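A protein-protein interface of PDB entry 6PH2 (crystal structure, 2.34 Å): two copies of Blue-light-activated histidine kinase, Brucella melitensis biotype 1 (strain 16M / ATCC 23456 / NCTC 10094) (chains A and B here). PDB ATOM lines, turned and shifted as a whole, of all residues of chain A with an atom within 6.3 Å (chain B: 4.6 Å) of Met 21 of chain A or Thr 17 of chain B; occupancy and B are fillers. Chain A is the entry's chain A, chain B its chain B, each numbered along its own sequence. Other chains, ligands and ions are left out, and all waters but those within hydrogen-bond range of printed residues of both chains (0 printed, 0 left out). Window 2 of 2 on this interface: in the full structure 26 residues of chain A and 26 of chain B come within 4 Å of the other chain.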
ATOM      1  N   ALA A  13     -14.909  -4.796   1.657  1.00  0.00           N
ATOM      2  CA  ALA A  13     -14.987  -5.889   0.697  1.00  0.00           C
ATOM      3  C   ALA A  13     -13.707  -6.735   0.756  1.00  0.00           C
ATOM      4  O   ALA A  13     -13.772  -7.961   0.841  1.00  0.00           O
ATOM      5  CB  ALA A  13     -15.206  -5.341  -0.699  1.00  0.00           C
ATOM      6  N   VAL A  14     -12.549  -6.062   0.736  1.00  0.00           N
ATOM      7  CA  VAL A  14     -11.289  -6.781   0.710  1.00  0.00           C
ATOM      8  C   VAL A  14     -10.969  -7.330   2.107  1.00  0.00           C
ATOM      9  O   VAL A  14     -10.438  -8.420   2.209  1.00  0.00           O
ATOM     10  CB  VAL A  14     -10.115  -6.020   0.067  1.00  0.00           C
ATOM     11  CG1 VAL A  14     -10.532  -5.091  -1.049  1.00  0.00           C
ATOM     12  CG2 VAL A  14      -9.263  -5.313   1.084  1.00  0.00           C
ATOM     13  N   THR A  17     -13.625 -10.608   2.382  1.00  0.00           N
ATOM     14  CA  THR A  17     -13.573 -11.717   1.404  1.00  0.00           C
ATOM     15  C   THR A  17     -12.706 -12.869   1.924  1.00  0.00           C
ATOM     16  O   THR A  17     -11.786 -12.674   2.700  1.00  0.00           O
ATOM     17  CB  THR A  17     -13.012 -11.257   0.052  1.00  0.00           C
ATOM     18  OG1 THR A  17     -13.069 -12.341  -0.882  1.00  0.00           O
ATOM     19  CG2 THR A  17     -11.582 -10.761   0.141  1.00  0.00           C
ATOM     20  N   MET A  19     -11.047 -14.666  -0.270  1.00  0.00           N
ATOM     21  CA  MET A  19      -9.944 -14.655  -1.248  1.00  0.00           C
ATOM     22  C   MET A  19      -8.748 -13.873  -0.681  1.00  0.00           C
ATOM     23  O   MET A  19      -8.880 -12.678  -0.403  1.00  0.00           O
ATOM     24  CB  MET A  19     -10.403 -13.999  -2.556  1.00  0.00           C
ATOM     25  CG  MET A  19      -9.341 -14.001  -3.655  1.00  0.00           C
ATOM     26  SD  MET A  19      -8.992 -15.652  -4.410  1.00  0.00           S
ATOM     27  CE  MET A  19      -9.688 -15.446  -6.053  1.00  0.00           C
ATOM     28  N   PRO A  20      -7.574 -14.526  -0.503  1.00  0.00           N
ATOM     29  CA  PRO A  20      -6.382 -13.795  -0.017  1.00  0.00           C
ATOM     30  C   PRO A  20      -5.975 -12.646  -0.954  1.00  0.00           C
ATOM     31  O   PRO A  20      -6.004 -12.840  -2.201  1.00  0.00           O
ATOM     32  CB  PRO A  20      -5.289 -14.871   0.016  1.00  0.00           C
ATOM     33  CG  PRO A  20      -6.042 -16.123   0.324  1.00  0.00           C
ATOM     34  CD  PRO A  20      -7.288 -15.964  -0.528  1.00  0.00           C
ATOM     35  N   MET A  21      -5.615 -11.491  -0.385  1.00  0.00           N
ATOM     36  CA  MET A  21      -5.255 -10.326  -1.196  1.00  0.00           C
ATOM     37  C   MET A  21      -4.137  -9.519  -0.534  1.00  0.00           C
ATOM     38  O   MET A  21      -4.132  -9.364   0.693  1.00  0.00           O
ATOM     39  CB  MET A  21      -6.462  -9.404  -1.376  1.00  0.00           C
ATOM     40  CG  MET A  21      -7.544  -9.996  -2.232  1.00  0.00           C
ATOM     41  SD  MET A  21      -8.720  -8.791  -2.778  1.00  0.00           S
ATOM     42  CE  MET A  21      -9.697  -9.795  -3.899  1.00  0.00           C
ATOM     43  N   LEU A  22      -3.228  -8.974  -1.362  1.00  0.00           N
ATOM     44  CA  LEU A  22      -2.154  -8.053  -0.895  1.00  0.00           C
ATOM     45  C   LEU A  22      -2.188  -6.745  -1.678  1.00  0.00           C
ATOM     46  O   LEU A  22      -2.471  -6.735  -2.886  1.00  0.00           O
ATOM     47  CB  LEU A  22      -0.782  -8.690  -1.113  1.00  0.00           C
ATOM     48  CG  LEU A  22      -0.444  -9.911  -0.269  1.00  0.00           C
ATOM     49  CD1 LEU A  22       0.922 -10.445  -0.683  1.00  0.00           C
ATOM     50  CD2 LEU A  22      -0.493  -9.597   1.234  1.00  0.00           C
ATOM     51  N   ILE A  23      -1.843  -5.658  -1.006  1.00  0.00           N
ATOM     52  CA  ILE A  23      -1.538  -4.407  -1.698  1.00  0.00           C
ATOM     53  C   ILE A  23      -0.096  -4.024  -1.369  1.00  0.00           C
ATOM     54  O   ILE A  23       0.301  -4.085  -0.199  1.00  0.00           O
ATOM     55  CB  ILE A  23      -2.523  -3.304  -1.281  1.00  0.00           C
ATOM     56  CG1 ILE A  23      -3.977  -3.751  -1.462  1.00  0.00           C
ATOM     57  CG2 ILE A  23      -2.238  -2.008  -2.013  1.00  0.00           C
ATOM     58  CD1 ILE A  23      -4.969  -2.914  -0.704  1.00  0.00           C
ATOM     59  N   PHE A  35      -0.724  -3.680   2.733  1.00  0.00           N
ATOM     60  CA  PHE A  35      -1.962  -4.256   3.257  1.00  0.00           C
ATOM     61  C   PHE A  35      -2.015  -5.753   2.944  1.00  0.00           C
ATOM     62  O   PHE A  35      -1.752  -6.172   1.809  1.00  0.00           O
ATOM     63  CB  PHE A  35      -3.198  -3.571   2.673  1.00  0.00           C
ATOM     64  CG  PHE A  35      -4.498  -4.136   3.187  1.00  0.00           C
ATOM     65  CD1 PHE A  35      -4.967  -3.797   4.447  1.00  0.00           C
ATOM     66  CD2 PHE A  35      -5.227  -5.050   2.434  1.00  0.00           C
ATOM     67  CE1 PHE A  35      -6.143  -4.346   4.934  1.00  0.00           C
ATOM     68  CE2 PHE A  35      -6.406  -5.590   2.920  1.00  0.00           C
ATOM     69  CZ  PHE A  35      -6.869  -5.225   4.163  1.00  0.00           C
ATOM     70  N   ALA A  36      -2.381  -6.533   3.963  1.00  0.00           N
ATOM     71  CA  ALA A  36      -2.701  -7.946   3.782  1.00  0.00           C
ATOM     72  C   ALA A  36      -4.022  -8.248   4.488  1.00  0.00           C
ATOM     73  O   ALA A  36      -4.178  -7.903   5.655  1.00  0.00           O
ATOM     74  CB  ALA A  36      -1.587  -8.796   4.317  1.00  0.00           C
ATOM     75  N   ASN A  37      -4.956  -8.900   3.783  1.00  0.00           N
ATOM     76  CA  ASN A  37      -6.292  -9.161   4.350  1.00  0.00           C
ATOM     77  C   ASN A  37      -6.208 -10.402   5.247  1.00  0.00           C
ATOM     78  O   ASN A  37      -5.255 -11.156   5.200  1.00  0.00           O
ATOM     79  CB  ASN A  37      -7.405  -9.261   3.302  1.00  0.00           C
ATOM     80  CG  ASN A  37      -7.304 -10.444   2.360  1.00  0.00           C
ATOM     81  OD1 ASN A  37      -6.484 -11.328   2.539  1.00  0.00           O
ATOM     82  ND2 ASN A  37      -8.151 -10.473   1.345  1.00  0.00           N
ATOM     83  N   ALA A  39      -7.641 -13.116   5.007  1.00  0.00           N
ATOM     84  CA  ALA A  39      -7.652 -14.364   4.223  1.00  0.00           C
ATOM     85  C   ALA A  39      -6.211 -14.777   3.888  1.00  0.00           C
ATOM     86  O   ALA A  39      -5.872 -15.970   3.852  1.00  0.00           O
ATOM     87  CB  ALA A  39      -8.481 -14.215   2.963  1.00  0.00           C
ATOM     88  N   PHE A  40      -5.384 -13.778   3.610  1.00  0.00           N
ATOM     89  CA  PHE A  40      -3.992 -14.017   3.295  1.00  0.00           C
ATOM     90  C   PHE A  40      -3.269 -14.519   4.546  1.00  0.00           C
ATOM     91  O   PHE A  40      -2.450 -15.409   4.457  1.00  0.00           O
ATOM     92  CB  PHE A  40      -3.329 -12.749   2.759  1.00  0.00           C
ATOM     93  CG  PHE A  40      -1.863 -12.905   2.455  1.00  0.00           C
ATOM     94  CD1 PHE A  40      -1.437 -13.366   1.221  1.00  0.00           C
ATOM     95  CD2 PHE A  40      -0.909 -12.617   3.430  1.00  0.00           C
ATOM     96  CE1 PHE A  40      -0.084 -13.523   0.959  1.00  0.00           C
ATOM     97  CE2 PHE A  40       0.440 -12.787   3.170  1.00  0.00           C
ATOM     98  CZ  PHE A  40       0.847 -13.235   1.933  1.00  0.00           C
ATOM     99  N   HIS A 101      -2.230 -13.680  -8.903  1.00  0.00           N
ATOM    100  CA  HIS A 101      -2.785 -12.741  -9.874  1.00  0.00           C
ATOM    101  C   HIS A 101      -2.410 -11.329  -9.428  1.00  0.00           C
ATOM    102  O   HIS A 101      -2.777 -10.914  -8.350  1.00  0.00           O
ATOM    103  CB  HIS A 101      -4.293 -12.994  -9.993  1.00  0.00           C
ATOM    104  CG  HIS A 101      -5.073 -11.973 -10.740  1.00  0.00           C
ATOM    105  ND1 HIS A 101      -4.959 -11.784 -12.106  1.00  0.00           N
ATOM    106  CD2 HIS A 101      -6.025 -11.127 -10.306  1.00  0.00           C
ATOM    107  CE1 HIS A 101      -5.819 -10.852 -12.485  1.00  0.00           C
ATOM    108  NE2 HIS A 101      -6.503 -10.440 -11.392  1.00  0.00           N
ATOM    109  N   SER A 103      -1.998  -7.173 -10.411  1.00  0.00           N
ATOM    110  CA  SER A 103      -2.380  -6.094 -11.291  1.00  0.00           C
ATOM    111  C   SER A 103      -1.727  -4.804 -10.793  1.00  0.00           C
ATOM    112  O   SER A 103      -1.752  -4.519  -9.593  1.00  0.00           O
ATOM    113  CB  SER A 103      -3.890  -5.924 -11.364  1.00  0.00           C
ATOM    114  OG  SER A 103      -4.583  -7.158 -11.560  1.00  0.00           O
ATOM    115  N   SER A 117      -2.914  -7.834  -5.547  1.00  0.00           N
ATOM    116  CA  SER A 117      -2.840  -9.221  -5.877  1.00  0.00           C
ATOM    117  C   SER A 117      -3.969 -10.019  -5.217  1.00  0.00           C
ATOM    118  O   SER A 117      -4.492  -9.647  -4.174  1.00  0.00           O
ATOM    119  CB  SER A 117      -1.515  -9.765  -5.462  1.00  0.00           C
ATOM    120  OG  SER A 117      -1.425  -9.845  -4.046  1.00  0.00           O
ATOM    121  N   SER A 118      -4.269 -11.142  -5.869  1.00  0.00           N
ATOM    122  CA  SER A 118      -4.965 -12.306  -5.308  1.00  0.00           C
ATOM    123  C   SER A 118      -3.977 -13.472  -5.186  1.00  0.00           C
ATOM    124  O   SER A 118      -3.025 -13.606  -5.974  1.00  0.00           O
ATOM    125  CB  SER A 118      -6.139 -12.724  -6.160  1.00  0.00           C
ATOM    126  OG  SER A 118      -6.955 -11.618  -6.533  1.00  0.00           O
ATOM    127  N   GLN A 119      -4.223 -14.315  -4.198  1.00  0.00           N
ATOM    128  CA  GLN A 119      -3.444 -15.515  -3.987  1.00  0.00           C
ATOM    129  C   GLN A 119      -4.413 -16.641  -3.657  1.00  0.00           C
ATOM    130  O   GLN A 119      -5.376 -16.398  -2.947  1.00  0.00           O
ATOM    131  CB  GLN A 119      -2.468 -15.342  -2.825  1.00  0.00           C
ATOM    132  CG  GLN A 119      -1.188 -14.593  -3.189  1.00  0.00           C
ATOM    133  CD  GLN A 119      -1.244 -13.095  -3.007  1.00  0.00           C
ATOM    134  OE1 GLN A 119      -2.272 -12.513  -2.660  1.00  0.00           O
ATOM    135  NE2 GLN A 119      -0.121 -12.451  -3.256  1.00  0.00           N
ATOM    136  N   ALA B  13      -8.547  -3.175  -6.173  1.00  0.00           N
ATOM    137  CA  ALA B  13      -8.484  -4.582  -5.777  1.00  0.00           C
ATOM    138  C   ALA B  13      -9.770  -5.307  -6.200  1.00  0.00           C
ATOM    139  O   ALA B  13      -9.731  -6.385  -6.798  1.00  0.00           O
ATOM    140  CB  ALA B  13      -8.259  -4.689  -4.294  1.00  0.00           C
ATOM    141  N   VAL B  14     -10.911  -4.695  -5.897  1.00  0.00           N
ATOM    142  CA  VAL B  14     -12.220  -5.263  -6.186  1.00  0.00           C
ATOM    143  C   VAL B  14     -12.499  -5.226  -7.694  1.00  0.00           C
ATOM    144  O   VAL B  14     -13.060  -6.171  -8.241  1.00  0.00           O
ATOM    145  CB  VAL B  14     -13.302  -4.514  -5.394  1.00  0.00           C
ATOM    146  CG1 VAL B  14     -14.706  -4.929  -5.809  1.00  0.00           C
ATOM    147  CG2 VAL B  14     -13.101  -4.674  -3.892  1.00  0.00           C
ATOM    148  N   GLU B  15     -12.123  -4.152  -8.368  1.00  0.00           N
ATOM    149  CA  GLU B  15     -12.406  -4.038  -9.793  1.00  0.00           C
ATOM    150  C   GLU B  15     -11.603  -5.089 -10.575  1.00  0.00           C
ATOM    151  O   GLU B  15     -12.077  -5.570 -11.589  1.00  0.00           O
ATOM    152  CB  GLU B  15     -12.113  -2.618 -10.284  1.00  0.00           C
ATOM    153  CG  GLU B  15     -13.041  -2.149 -11.401  1.00  0.00           C
ATOM    154  CD  GLU B  15     -13.509  -0.694 -11.304  1.00  0.00           C
ATOM    155  OE1 GLU B  15     -13.481   0.008 -12.342  1.00  0.00           O
ATOM    156  OE2 GLU B  15     -13.899  -0.252 -10.191  1.00  0.00           O
ATOM    157  N   PHE B  16     -10.419  -5.482 -10.089  1.00  0.00           N
ATOM    158  CA  PHE B  16      -9.458  -6.268 -10.900  1.00  0.00           C
ATOM    159  C   PHE B  16      -9.465  -7.760 -10.526  1.00  0.00           C
ATOM    160  O   PHE B  16      -9.066  -8.600 -11.351  1.00  0.00           O
ATOM    161  CB  PHE B  16      -8.048  -5.670 -10.798  1.00  0.00           C
ATOM    162  CG  PHE B  16      -7.850  -4.366 -11.538  1.00  0.00           C
ATOM    163  CD1 PHE B  16      -8.342  -4.176 -12.825  1.00  0.00           C
ATOM    164  CD2 PHE B  16      -7.131  -3.328 -10.962  1.00  0.00           C
ATOM    165  CE1 PHE B  16      -8.153  -2.975 -13.493  1.00  0.00           C
ATOM    166  CE2 PHE B  16      -6.923  -2.134 -11.641  1.00  0.00           C
ATOM    167  CZ  PHE B  16      -7.447  -1.952 -12.898  1.00  0.00           C
ATOM    168  N   THR B  17      -9.895  -8.115  -9.323  1.00  0.00           N
ATOM    169  CA  THR B  17      -9.998  -9.531  -8.926  1.00  0.00           C
ATOM    170  C   THR B  17     -10.875 -10.315  -9.904  1.00  0.00           C
ATOM    171  O   THR B  17     -11.786  -9.768 -10.513  1.00  0.00           O
ATOM    172  CB  THR B  17     -10.570  -9.687  -7.510  1.00  0.00           C
ATOM    173  OG1 THR B  17     -10.566 -11.061  -7.148  1.00  0.00           O
ATOM    174  CG2 THR B  17     -11.985  -9.180  -7.364  1.00  0.00           C
ATOM    175  N   LEU B  18     -10.605 -11.613 -10.000  1.00  0.00           N
ATOM    176  CA  LEU B  18     -11.365 -12.540 -10.849  1.00  0.00           C
ATOM    177  C   LEU B  18     -12.545 -13.133 -10.068  1.00  0.00           C
ATOM    178  O   LEU B  18     -13.374 -13.842 -10.656  1.00  0.00           O
ATOM    179  CB  LEU B  18     -10.445 -13.673 -11.316  1.00  0.00           C
ATOM    180  CG  LEU B  18      -9.261 -13.287 -12.206  1.00  0.00           C
ATOM    181  CD1 LEU B  18      -8.439 -14.532 -12.514  1.00  0.00           C
ATOM    182  CD2 LEU B  18      -9.712 -12.606 -13.509  1.00  0.00           C
ATOM    183  N   MET B  19     -12.582 -12.872  -8.755  1.00  0.00           N
ATOM    184  CA  MET B  19     -13.663 -13.308  -7.854  1.00  0.00           C
ATOM    185  C   MET B  19     -14.839 -12.328  -7.977  1.00  0.00           C
ATOM    186  O   MET B  19     -14.695 -11.140  -7.696  1.00  0.00           O
ATOM    187  CB  MET B  19     -13.154 -13.321  -6.406  1.00  0.00           C
ATOM    188  CG  MET B  19     -14.164 -13.724  -5.367  1.00  0.00           C
ATOM    189  SD  MET B  19     -14.441 -15.516  -5.314  1.00  0.00           S
ATOM    190  CE  MET B  19     -14.062 -15.848  -3.592  1.00  0.00           C
ATOM    191  N   MET B  21     -17.942 -10.071  -7.032  1.00  0.00           N
ATOM    192  CA  MET B  21     -18.224  -9.379  -5.769  1.00  0.00           C
ATOM    193  C   MET B  21     -19.364  -8.371  -5.947  1.00  0.00           C
ATOM    194  O   MET B  21     -19.439  -7.716  -6.988  1.00  0.00           O
ATOM    195  CB  MET B  21     -16.996  -8.623  -5.263  1.00  0.00           C
ATOM    196  CG  MET B  21     -15.881  -9.527  -4.814  1.00  0.00           C
ATOM    197  SD  MET B  21     -14.495  -8.568  -4.134  1.00  0.00           S
ATOM    198  CE  MET B  21     -14.979  -8.520  -2.413  1.00  0.00           C
ATOM    199  N   ASN B  37     -18.744  -5.929  -9.613  1.00  0.00           N
ATOM    200  CA  ASN B  37     -17.421  -5.873 -10.256  1.00  0.00           C
ATOM    201  C   ASN B  37     -17.487  -6.560 -11.619  1.00  0.00           C
ATOM    202  O   ASN B  37     -18.419  -7.257 -11.908  1.00  0.00           O
ATOM    203  CB  ASN B  37     -16.291  -6.405  -9.341  1.00  0.00           C
ATOM    204  CG  ASN B  37     -16.324  -7.895  -9.084  1.00  0.00           C
ATOM    205  OD1 ASN B  37     -17.160  -8.611  -9.623  1.00  0.00           O
ATOM    206  ND2 ASN B  37     -15.426  -8.372  -8.241  1.00  0.00           N
ATOM    207  N   ALA B  39     -16.085  -9.114 -12.664  1.00  0.00           N
ATOM    208  CA  ALA B  39     -16.065 -10.569 -12.538  1.00  0.00           C
ATOM    209  C   ALA B  39     -17.497 -11.083 -12.386  1.00  0.00           C
ATOM    210  O   ALA B  39     -17.846 -12.154 -12.911  1.00  0.00           O
ATOM    211  CB  ALA B  39     -15.192 -10.995 -11.368  1.00  0.00           C
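O of Phe 16 of chain B sits at hydrogen-bond distance from NE2 of His 101 of chain A.
O of His 101 of chain A lies within hydrogen-bond range of N of Ser 118 of chain A (2.9 Å). O of Val 14 of chain B sits at hydrogen-bond distance from ND2 of Asn 37 of chain B, 3.2 Å away. The backbone NH of Met 21 of chain A is in hydrogen-bond range of the side-chain amide oxygen of Asn 37 of chain A (3.1 Å). The backbone carbonyl oxygen (O) of Val 14 of chain A is in hydrogen-bond range of the side-chain amide nitrogen (ND2) of Asn 37 of chain A (3.2 Å). The side-chain amide oxygen (OD1) of Asn 37 of chain B lies within hydrogen-bond range of the backbone NH (N) of Met 21 of chain B, 3.1 Å away. N of Met 19 of chain B sits at hydrogen-bond distance from OG1 of Thr 17 of chain B (3.2 Å).
Among the printed residues, merely in contact across the chains: Ala 13 of chain A with Met 21 of chain B, Met 21 of chain A with Thr 17 of chain B, Ser 118 of chain A with Thr 17 of chain B, Ser 103 of chain A with Phe 16 of chain B, Val 14 of chain A with Val 14 of chain B, Ala 13 of chain A with Val 14 of chain B and Val 14 of chain A with Ala 13 of chain B.
Met 21 of chain A touches one residue of chain B. Of the printed residues of chain B, His 101 of chain A touches Phe 16. Printed residues of chain B within 4 Å of Ser 103 of chain A: Phe 16 (3.8 Å). Of the printed residues of chain A, Ala 13 of chain B touches Val 14. Of the printed residues of chain A, Val 14 of chain B touches Ala 13 (3.9 Å) and Val 14 (3.9 Å). Of the printed residues of chain A, Phe 16 of chain B touches His 101 and Ser 103.
Printed residues of chain B that touch a printed residue of chain A: Ala 13, Val 14, Phe 16, Thr 17 and Met 21. Among the printed residues, no Asp or Glu carboxylate lies within 4 Å of a Lys or Arg side-chain nitrogen of the other chain.
Ala 13 of chain A touches Val 14 of chain B, and with the chains exchanged Val 14 of chain A touches Ala 13 of chain B. Ala 13 of chain A touches Met 21 of chain B, but with the chains exchanged Met 21 of chain A does not touch Ala 13 of chain B (4.4 Å). Val 14 of chain B touches its own counterpart, Val 14 of chain A. Met 21 of chain A touches Thr 17 of chain B, but with the chains exchanged Thr 17 of chain A does not touch Met 21 of chain B (4.2 Å). Positions printed for both chains: 13, 14, 17, 19, 21, 37 and 39. Of the 8 pairs that touch across the chains among the printed residues, 3 have their exchanged pair printed and touching as well.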
